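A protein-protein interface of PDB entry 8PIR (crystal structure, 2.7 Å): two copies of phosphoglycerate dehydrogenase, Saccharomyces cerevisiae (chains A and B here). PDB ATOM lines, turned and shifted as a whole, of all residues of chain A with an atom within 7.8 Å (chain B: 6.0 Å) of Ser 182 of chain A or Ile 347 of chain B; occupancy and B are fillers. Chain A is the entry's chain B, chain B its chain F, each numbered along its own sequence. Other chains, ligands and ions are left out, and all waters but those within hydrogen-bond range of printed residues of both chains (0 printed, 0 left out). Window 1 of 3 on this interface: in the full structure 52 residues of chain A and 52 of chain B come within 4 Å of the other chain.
The backbone carbonyl oxygen of Ile 346 of chain B sits close to a ring nitrogen (NE2) of His 186 of chain A (3.4 Å).
The side-chain hydroxyl of Ser 182 of chain A lies within hydrogen-bond range of the backbone NH of Leu 348 of chain B, at 3.1 Å.
The backbone NH (N) of Ile 347 of chain B sits at hydrogen-bond distance from the backbone carbonyl oxygen (O) of Ala 312 of chain B.
The side-chain amide oxygen (OE1) of Gln 177 of chain A sits at hydrogen-bond distance from the guanidinium group (NH1) of Arg 181 of chain A, at 3.1 Å.
The side-chain carboxylate (OD1) of Asp 315 of chain B sits at hydrogen-bond distance from the side-chain hydroxyl (OG1) of Thr 349 of chain B, 2.7 Å away.
The backbone NH (N) of Leu 314 of chain B lies within hydrogen-bond range of the backbone carbonyl oxygen (O) of Ile 347 of chain B (2.9 Å).
The backbone carbonyl oxygen (O) of Leu 314 of chain B is in hydrogen-bond range of the side-chain hydroxyl (OH) of Tyr 317 of chain B (3.1 Å).
A ring nitrogen (ND1) of His 186 of chain A sits at hydrogen-bond distance from the backbone carbonyl oxygen of Ser 182 of chain A.
Among the printed residues, merely in contact across the chains: Leu 185 of chain A with Thr 349 of chain B (3.1 Å), Leu 185 of chain A with Leu 348 of chain B (3.2 Å), Leu 185 of chain A with Pro 350 of chain B (3.3 Å), Ser 182 of chain A with Ile 347 of chain B (3.6 Å), Leu 185 of chain A with Tyr 317 of chain B (3.7 Å), Arg 181 of chain A with Pro 350 of chain B (3.8 Å), Arg 181 of chain A with Leu 348 of chain B (3.8 Å), His 186 of chain A with Leu 348 of chain B (3.9 Å) and Ser 182 of chain A with Ile 346 of chain B (3.998 Å).
Printed residues of chain B within 4 Å of Arg 181 of chain A: Leu 348 and Pro 350.
Of the printed residues of chain B, Ser 182 of chain A touches Ile 346 (3.998 Å), Ile 347 (3.6 Å) and Leu 348 (3.0 Å).
Glu 184 of chain A touches none of the printed residues of chain B.
Printed residues of chain B within 4 Å of His 186 of chain A: Ile 346 (3.1 Å) and Leu 348 (3.9 Å).
Printed residues of chain A within 4 Å of Tyr 317 of chain B: Leu 185 (3.7 Å).
Of the printed residues of chain A, Ile 346 of chain B touches Ser 182 and His 186.
Ile 347 of chain B touches just one residue of chain A: Ser 182.
Of the printed residues of chain A, Pro 350 of chain B touches Arg 181 (3.8 Å) and Leu 185 (3.3 Å).
Of the 15 printed residues of chain B, 6 touch a printed residue of chain A.
Hydrophobic or aromatic side chains of chain B that line the printed part of chain A: Tyr 317, Ile 347, Leu 348 and Pro 350.
Of the 13 printed residues of chain A, 4 touch a printed residue of chain B.
Printed residues of chain A that touch a printed residue of chain B: Arg 181, Ser 182, Leu 185 and His 186.
Hydrophobic or aromatic side chains of chain A that line the printed part of chain B: Leu 185 and His 186.
Among the printed residues, no Asp or Glu carboxylate lies within 4 Å of a Lys or Arg side-chain nitrogen of the other chain.
No position is printed for both chains.
Of the 11 pairs that touch across the chains among the printed residues, none has its exchanged pair printed and touching as well.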
ATOM      1  N   GLN A 177      19.845 -35.708  24.106  1.00  0.00           N
ATOM      2  CA  GLN A 177      18.992 -34.893  23.194  1.00  0.00           C
ATOM      3  C   GLN A 177      19.870 -34.160  22.167  1.00  0.00           C
ATOM      4  O   GLN A 177      19.615 -32.964  21.929  1.00  0.00           O
ATOM      5  CB  GLN A 177      18.157 -33.874  23.979  1.00  0.00           C
ATOM      6  CG  GLN A 177      17.429 -34.462  25.183  1.00  0.00           C
ATOM      7  CD  GLN A 177      16.618 -33.434  25.936  1.00  0.00           C
ATOM      8  OE1 GLN A 177      16.571 -32.257  25.584  1.00  0.00           O
ATOM      9  NE2 GLN A 177      15.968 -33.876  26.999  1.00  0.00           N
ATOM     10  N   LEU A 178      20.823 -34.858  21.539  1.00  0.00           N
ATOM     11  CA  LEU A 178      21.790 -34.258  20.581  1.00  0.00           C
ATOM     12  C   LEU A 178      21.040 -33.636  19.402  1.00  0.00           C
ATOM     13  O   LEU A 178      21.389 -32.504  19.028  1.00  0.00           O
ATOM     14  CB  LEU A 178      22.760 -35.326  20.075  1.00  0.00           C
ATOM     15  CG  LEU A 178      23.989 -35.551  20.945  1.00  0.00           C
ATOM     16  CD1 LEU A 178      23.569 -36.070  22.311  1.00  0.00           C
ATOM     17  CD2 LEU A 178      24.949 -36.516  20.266  1.00  0.00           C
ATOM     18  N   GLY A 179      20.200 -34.426  18.728  1.00  0.00           N
ATOM     19  CA  GLY A 179      19.400 -33.986  17.570  1.00  0.00           C
ATOM     20  C   GLY A 179      18.741 -32.640  17.826  1.00  0.00           C
ATOM     21  O   GLY A 179      18.942 -31.725  17.014  1.00  0.00           O
ATOM     22  N   ASP A 180      18.038 -32.506  18.955  1.00  0.00           N
ATOM     23  CA  ASP A 180      17.301 -31.271  19.344  1.00  0.00           C
ATOM     24  C   ASP A 180      18.307 -30.125  19.498  1.00  0.00           C
ATOM     25  O   ASP A 180      18.009 -29.011  19.032  1.00  0.00           O
ATOM     26  CB  ASP A 180      16.487 -31.461  20.630  1.00  0.00           C
ATOM     27  CG  ASP A 180      15.309 -32.422  20.497  1.00  0.00           C
ATOM     28  OD1 ASP A 180      14.877 -32.681  19.354  1.00  0.00           O
ATOM     29  OD2 ASP A 180      14.849 -32.933  21.542  1.00  0.00           O
ATOM     30  N   ARG A 181      19.412 -30.372  20.203  1.00  0.00           N
ATOM     31  CA  ARG A 181      20.472 -29.364  20.459  1.00  0.00           C
ATOM     32  C   ARG A 181      20.998 -28.828  19.124  1.00  0.00           C
ATOM     33  O   ARG A 181      21.117 -27.603  18.995  1.00  0.00           O
ATOM     34  CB  ARG A 181      21.607 -29.980  21.279  1.00  0.00           C
ATOM     35  CG  ARG A 181      21.253 -30.209  22.737  1.00  0.00           C
ATOM     36  CD  ARG A 181      20.832 -28.925  23.433  1.00  0.00           C
ATOM     37  NE  ARG A 181      19.388 -28.756  23.404  1.00  0.00           N
ATOM     38  CZ  ARG A 181      18.519 -29.486  24.101  1.00  0.00           C
ATOM     39  NH1 ARG A 181      18.938 -30.441  24.916  1.00  0.00           N
ATOM     40  NH2 ARG A 181      17.223 -29.293  23.927  1.00  0.00           N
ATOM     41  N   SER A 182      21.251 -29.708  18.150  1.00  0.00           N
ATOM     42  CA  SER A 182      21.879 -29.354  16.851  1.00  0.00           C
ATOM     43  C   SER A 182      20.866 -28.631  15.950  1.00  0.00           C
ATOM     44  O   SER A 182      21.280 -27.703  15.212  1.00  0.00           O
ATOM     45  CB  SER A 182      22.459 -30.565  16.180  1.00  0.00           C
ATOM     46  OG  SER A 182      23.365 -30.177  15.159  1.00  0.00           O
ATOM     47  N   ILE A 183      19.584 -29.002  16.033  1.00  0.00           N
ATOM     48  CA  ILE A 183      18.487 -28.357  15.254  1.00  0.00           C
ATOM     49  C   ILE A 183      18.294 -26.929  15.781  1.00  0.00           C
ATOM     50  O   ILE A 183      18.295 -26.000  14.962  1.00  0.00           O
ATOM     51  CB  ILE A 183      17.198 -29.200  15.309  1.00  0.00           C
ATOM     52  CG1 ILE A 183      17.268 -30.379  14.333  1.00  0.00           C
ATOM     53  CG2 ILE A 183      15.964 -28.343  15.056  1.00  0.00           C
ATOM     54  CD1 ILE A 183      16.352 -31.528  14.689  1.00  0.00           C
ATOM     55  N   GLU A 184      18.273 -26.761  17.105  1.00  0.00           N
ATOM     56  CA  GLU A 184      18.195 -25.439  17.781  1.00  0.00           C
ATOM     57  C   GLU A 184      19.301 -24.516  17.250  1.00  0.00           C
ATOM     58  O   GLU A 184      18.970 -23.402  16.817  1.00  0.00           O
ATOM     59  CB  GLU A 184      18.293 -25.601  19.297  1.00  0.00           C
ATOM     60  CG  GLU A 184      17.026 -26.148  19.936  1.00  0.00           C
ATOM     61  CD  GLU A 184      17.226 -26.659  21.353  1.00  0.00           C
ATOM     62  OE1 GLU A 184      18.380 -26.638  21.828  1.00  0.00           O
ATOM     63  OE2 GLU A 184      16.232 -27.062  21.986  1.00  0.00           O
ATOM     64  N   LEU A 185      20.572 -24.882  17.376  1.00  0.00           N
ATOM     65  CA  LEU A 185      21.687 -23.959  17.037  1.00  0.00           C
ATOM     66  C   LEU A 185      21.688 -23.624  15.555  1.00  0.00           C
ATOM     67  O   LEU A 185      22.132 -22.534  15.207  1.00  0.00           O
ATOM     68  CB  LEU A 185      23.011 -24.607  17.437  1.00  0.00           C
ATOM     69  CG  LEU A 185      23.231 -24.844  18.926  1.00  0.00           C
ATOM     70  CD1 LEU A 185      24.513 -25.619  19.137  1.00  0.00           C
ATOM     71  CD2 LEU A 185      23.320 -23.527  19.665  1.00  0.00           C
ATOM     72  N   HIS A 186      21.241 -24.548  14.731  1.00  0.00           N
ATOM     73  CA  HIS A 186      21.197 -24.350  13.259  1.00  0.00           C
ATOM     74  C   HIS A 186      20.172 -23.260  12.920  1.00  0.00           C
ATOM     75  O   HIS A 186      20.362 -22.583  11.897  1.00  0.00           O
ATOM     76  CB  HIS A 186      20.896 -25.674  12.548  1.00  0.00           C
ATOM     77  CG  HIS A 186      22.105 -26.498  12.255  1.00  0.00           C
ATOM     78  ND1 HIS A 186      22.632 -27.394  13.167  1.00  0.00           N
ATOM     79  CD2 HIS A 186      22.861 -26.604  11.139  1.00  0.00           C
ATOM     80  CE1 HIS A 186      23.675 -27.998  12.632  1.00  0.00           C
ATOM     81  NE2 HIS A 186      23.824 -27.544  11.381  1.00  0.00           N
ATOM     82  N   THR A 187      19.122 -23.120  13.744  1.00  0.00           N
ATOM     83  CA  THR A 187      18.075 -22.064  13.658  1.00  0.00           C
ATOM     84  C   THR A 187      18.522 -20.832  14.452  1.00  0.00           C
ATOM     85  O   THR A 187      17.756 -19.858  14.474  1.00  0.00           O
ATOM     86  CB  THR A 187      16.719 -22.551  14.190  1.00  0.00           C
ATOM     87  N   GLY A 188      19.643 -20.931  15.179  1.00  0.00           N
ATOM     88  CA  GLY A 188      20.284 -19.801  15.882  1.00  0.00           C
ATOM     89  C   GLY A 188      19.894 -19.729  17.353  1.00  0.00           C
ATOM     90  O   GLY A 188      20.299 -18.751  18.024  1.00  0.00           O
ATOM     91  N   THR A 189      19.187 -20.746  17.860  1.00  0.00           N
ATOM     92  CA  THR A 189      18.820 -20.885  19.295  1.00  0.00           C
ATOM     93  C   THR A 189      19.962 -21.564  20.068  1.00  0.00           C
ATOM     94  O   THR A 189      20.357 -22.688  19.687  1.00  0.00           O
ATOM     95  CB  THR A 189      17.512 -21.673  19.461  1.00  0.00           C
ATOM     96  OG1 THR A 189      16.470 -21.022  18.734  1.00  0.00           O
ATOM     97  CG2 THR A 189      17.121 -21.830  20.913  1.00  0.00           C
ATOM     98  N   GLY B 169      29.026 -40.976  20.807  1.00  0.00           N
ATOM     99  CA  GLY B 169      27.743 -40.700  20.136  1.00  0.00           C
ATOM    100  C   GLY B 169      27.945 -39.973  18.818  1.00  0.00           C
ATOM    101  O   GLY B 169      27.304 -40.345  17.821  1.00  0.00           O
ATOM    102  N   GLU B 170      28.867 -39.012  18.802  1.00  0.00           N
ATOM    103  CA  GLU B 170      29.093 -38.082  17.664  1.00  0.00           C
ATOM    104  C   GLU B 170      29.948 -38.764  16.599  1.00  0.00           C
ATOM    105  O   GLU B 170      29.712 -38.479  15.416  1.00  0.00           O
ATOM    106  CB  GLU B 170      29.735 -36.787  18.161  1.00  0.00           C
ATOM    107  CG  GLU B 170      28.736 -35.897  18.868  1.00  0.00           C
ATOM    108  CD  GLU B 170      29.284 -34.575  19.360  1.00  0.00           C
ATOM    109  OE1 GLU B 170      30.502 -34.512  19.632  1.00  0.00           O
ATOM    110  OE2 GLU B 170      28.483 -33.618  19.482  1.00  0.00           O
ATOM    111  N   SER B 173      27.373 -40.836  14.956  1.00  0.00           N
ATOM    112  CA  SER B 173      26.360 -39.958  14.320  1.00  0.00           C
ATOM    113  C   SER B 173      26.939 -39.374  13.024  1.00  0.00           C
ATOM    114  O   SER B 173      26.277 -39.490  11.984  1.00  0.00           O
ATOM    115  CB  SER B 173      25.898 -38.888  15.254  1.00  0.00           C
ATOM    116  OG  SER B 173      25.045 -37.976  14.580  1.00  0.00           O
ATOM    117  N   LEU B 174      28.209 -38.967  13.045  1.00  0.00           N
ATOM    118  CA  LEU B 174      28.926 -38.444  11.856  1.00  0.00           C
ATOM    119  C   LEU B 174      29.152 -39.571  10.849  1.00  0.00           C
ATOM    120  O   LEU B 174      29.047 -39.309   9.651  1.00  0.00           O
ATOM    121  CB  LEU B 174      30.263 -37.845  12.292  1.00  0.00           C
ATOM    122  CG  LEU B 174      30.179 -36.494  12.994  1.00  0.00           C
ATOM    123  CD1 LEU B 174      31.568 -36.037  13.408  1.00  0.00           C
ATOM    124  CD2 LEU B 174      29.506 -35.447  12.110  1.00  0.00           C
ATOM    125  N   ALA B 312      31.840 -32.738  10.897  1.00  0.00           N
ATOM    126  CA  ALA B 312      32.422 -32.155  12.127  1.00  0.00           C
ATOM    127  C   ALA B 312      31.345 -32.059  13.210  1.00  0.00           C
ATOM    128  O   ALA B 312      30.162 -31.937  12.868  1.00  0.00           O
ATOM    129  CB  ALA B 312      33.027 -30.807  11.827  1.00  0.00           C
ATOM    130  N   ALA B 313      31.747 -32.189  14.473  1.00  0.00           N
ATOM    131  CA  ALA B 313      30.915 -31.863  15.651  1.00  0.00           C
ATOM    132  C   ALA B 313      31.661 -30.834  16.502  1.00  0.00           C
ATOM    133  O   ALA B 313      32.806 -31.133  16.893  1.00  0.00           O
ATOM    134  CB  ALA B 313      30.600 -33.114  16.431  1.00  0.00           C
ATOM    135  N   LEU B 314      31.047 -29.665  16.728  1.00  0.00           N
ATOM    136  CA  LEU B 314      31.580 -28.582  17.594  1.00  0.00           C
ATOM    137  C   LEU B 314      30.657 -28.409  18.802  1.00  0.00           C
ATOM    138  O   LEU B 314      29.435 -28.329  18.603  1.00  0.00           O
ATOM    139  CB  LEU B 314      31.690 -27.290  16.775  1.00  0.00           C
ATOM    140  CG  LEU B 314      32.427 -27.431  15.443  1.00  0.00           C
ATOM    141  CD1 LEU B 314      32.445 -26.117  14.678  1.00  0.00           C
ATOM    142  CD2 LEU B 314      33.845 -27.937  15.658  1.00  0.00           C
ATOM    143  N   ASP B 315      31.232 -28.375  20.006  1.00  0.00           N
ATOM    144  CA  ASP B 315      30.505 -28.100  21.273  1.00  0.00           C
ATOM    145  C   ASP B 315      30.872 -26.699  21.781  1.00  0.00           C
ATOM    146  O   ASP B 315      30.190 -26.216  22.711  1.00  0.00           O
ATOM    147  CB  ASP B 315      30.821 -29.169  22.322  1.00  0.00           C
ATOM    148  CG  ASP B 315      29.853 -29.168  23.496  1.00  0.00           C
ATOM    149  OD1 ASP B 315      28.632 -29.009  23.255  1.00  0.00           O
ATOM    150  OD2 ASP B 315      30.327 -29.328  24.643  1.00  0.00           O
ATOM    151  N   TYR B 317      32.865 -22.702  20.859  1.00  0.00           N
ATOM    152  CA  TYR B 317      33.103 -21.697  19.800  1.00  0.00           C
ATOM    153  C   TYR B 317      33.876 -20.507  20.381  1.00  0.00           C
ATOM    154  O   TYR B 317      33.845 -20.330  21.599  1.00  0.00           O
ATOM    155  CB  TYR B 317      31.746 -21.287  19.239  1.00  0.00           C
ATOM    156  CG  TYR B 317      30.781 -22.422  19.018  1.00  0.00           C
ATOM    157  CD1 TYR B 317      30.755 -23.109  17.819  1.00  0.00           C
ATOM    158  CD2 TYR B 317      29.897 -22.809  20.009  1.00  0.00           C
ATOM    159  CE1 TYR B 317      29.878 -24.155  17.609  1.00  0.00           C
ATOM    160  CE2 TYR B 317      29.019 -23.858  19.817  1.00  0.00           C
ATOM    161  CZ  TYR B 317      29.008 -24.530  18.613  1.00  0.00           C
ATOM    162  OH  TYR B 317      28.141 -25.558  18.415  1.00  0.00           O
ATOM    163  N   ASN B 345      26.230 -32.468   7.429  1.00  0.00           N
ATOM    164  CA  ASN B 345      26.892 -33.402   8.383  1.00  0.00           C
ATOM    165  C   ASN B 345      27.786 -32.626   9.366  1.00  0.00           C
ATOM    166  O   ASN B 345      28.853 -33.154   9.736  1.00  0.00           O
ATOM    167  CB  ASN B 345      27.695 -34.484   7.655  1.00  0.00           C
ATOM    168  CG  ASN B 345      27.799 -35.768   8.452  1.00  0.00           C
ATOM    169  OD1 ASN B 345      26.925 -36.081   9.262  1.00  0.00           O
ATOM    170  ND2 ASN B 345      28.881 -36.504   8.253  1.00  0.00           N
ATOM    171  N   ILE B 346      27.312 -31.475   9.858  1.00  0.00           N
ATOM    172  CA  ILE B 346      27.944 -30.720  10.977  1.00  0.00           C
ATOM    173  C   ILE B 346      26.985 -30.715  12.170  1.00  0.00           C
ATOM    174  O   ILE B 346      25.899 -30.104  12.068  1.00  0.00           O
ATOM    175  CB  ILE B 346      28.355 -29.297  10.550  1.00  0.00           C
ATOM    176  CG1 ILE B 346      29.238 -29.317   9.297  1.00  0.00           C
ATOM    177  CG2 ILE B 346      29.035 -28.571  11.702  1.00  0.00           C
ATOM    178  N   ILE B 347      27.371 -31.400  13.253  1.00  0.00           N
ATOM    179  CA  ILE B 347      26.669 -31.360  14.568  1.00  0.00           C
ATOM    180  C   ILE B 347      27.172 -30.143  15.350  1.00  0.00           C
ATOM    181  O   ILE B 347      28.369 -30.091  15.655  1.00  0.00           O
ATOM    182  CB  ILE B 347      26.881 -32.671  15.349  1.00  0.00           C
ATOM    183  CG1 ILE B 347      26.541 -33.894  14.494  1.00  0.00           C
ATOM    184  CG2 ILE B 347      26.095 -32.652  16.651  1.00  0.00           C
ATOM    185  CD1 ILE B 347      27.118 -35.185  15.025  1.00  0.00           C
ATOM    186  N   LEU B 348      26.275 -29.211  15.666  1.00  0.00           N
ATOM    187  CA  LEU B 348      26.559 -28.046  16.538  1.00  0.00           C
ATOM    188  C   LEU B 348      25.796 -28.220  17.847  1.00  0.00           C
ATOM    189  O   LEU B 348      24.588 -28.499  17.787  1.00  0.00           O
ATOM    190  CB  LEU B 348      26.132 -26.764  15.820  1.00  0.00           C
ATOM    191  CG  LEU B 348      26.789 -26.526  14.464  1.00  0.00           C
ATOM    192  CD1 LEU B 348      26.317 -25.213  13.854  1.00  0.00           C
ATOM    193  CD2 LEU B 348      28.302 -26.541  14.584  1.00  0.00           C
ATOM    194  N   THR B 349      26.503 -28.167  18.972  1.00  0.00           N
ATOM    195  CA  THR B 349      25.884 -28.358  20.304  1.00  0.00           C
ATOM    196  C   THR B 349      26.251 -27.166  21.183  1.00  0.00           C
ATOM    197  O   THR B 349      27.315 -26.605  20.984  1.00  0.00           O
ATOM    198  CB  THR B 349      26.268 -29.713  20.901  1.00  0.00           C
ATOM    199  OG1 THR B 349      27.689 -29.798  20.902  1.00  0.00           O
ATOM    200  CG2 THR B 349      25.660 -30.889  20.172  1.00  0.00           C
ATOM    201  N   PRO B 350      25.386 -26.705  22.133  1.00  0.00           N
ATOM    202  CA  PRO B 350      25.647 -25.497  22.926  1.00  0.00           C
ATOM    203  C   PRO B 350      26.388 -25.765  24.242  1.00  0.00           C
ATOM    204  O   PRO B 350      25.768 -25.649  25.283  1.00  0.00           O
ATOM    205  CB  PRO B 350      24.252 -24.938  23.263  1.00  0.00           C
ATOM    206  CG  PRO B 350      23.263 -25.990  22.800  1.00  0.00           C
ATOM    207  CD  PRO B 350      24.074 -27.240  22.542  1.00  0.00           C
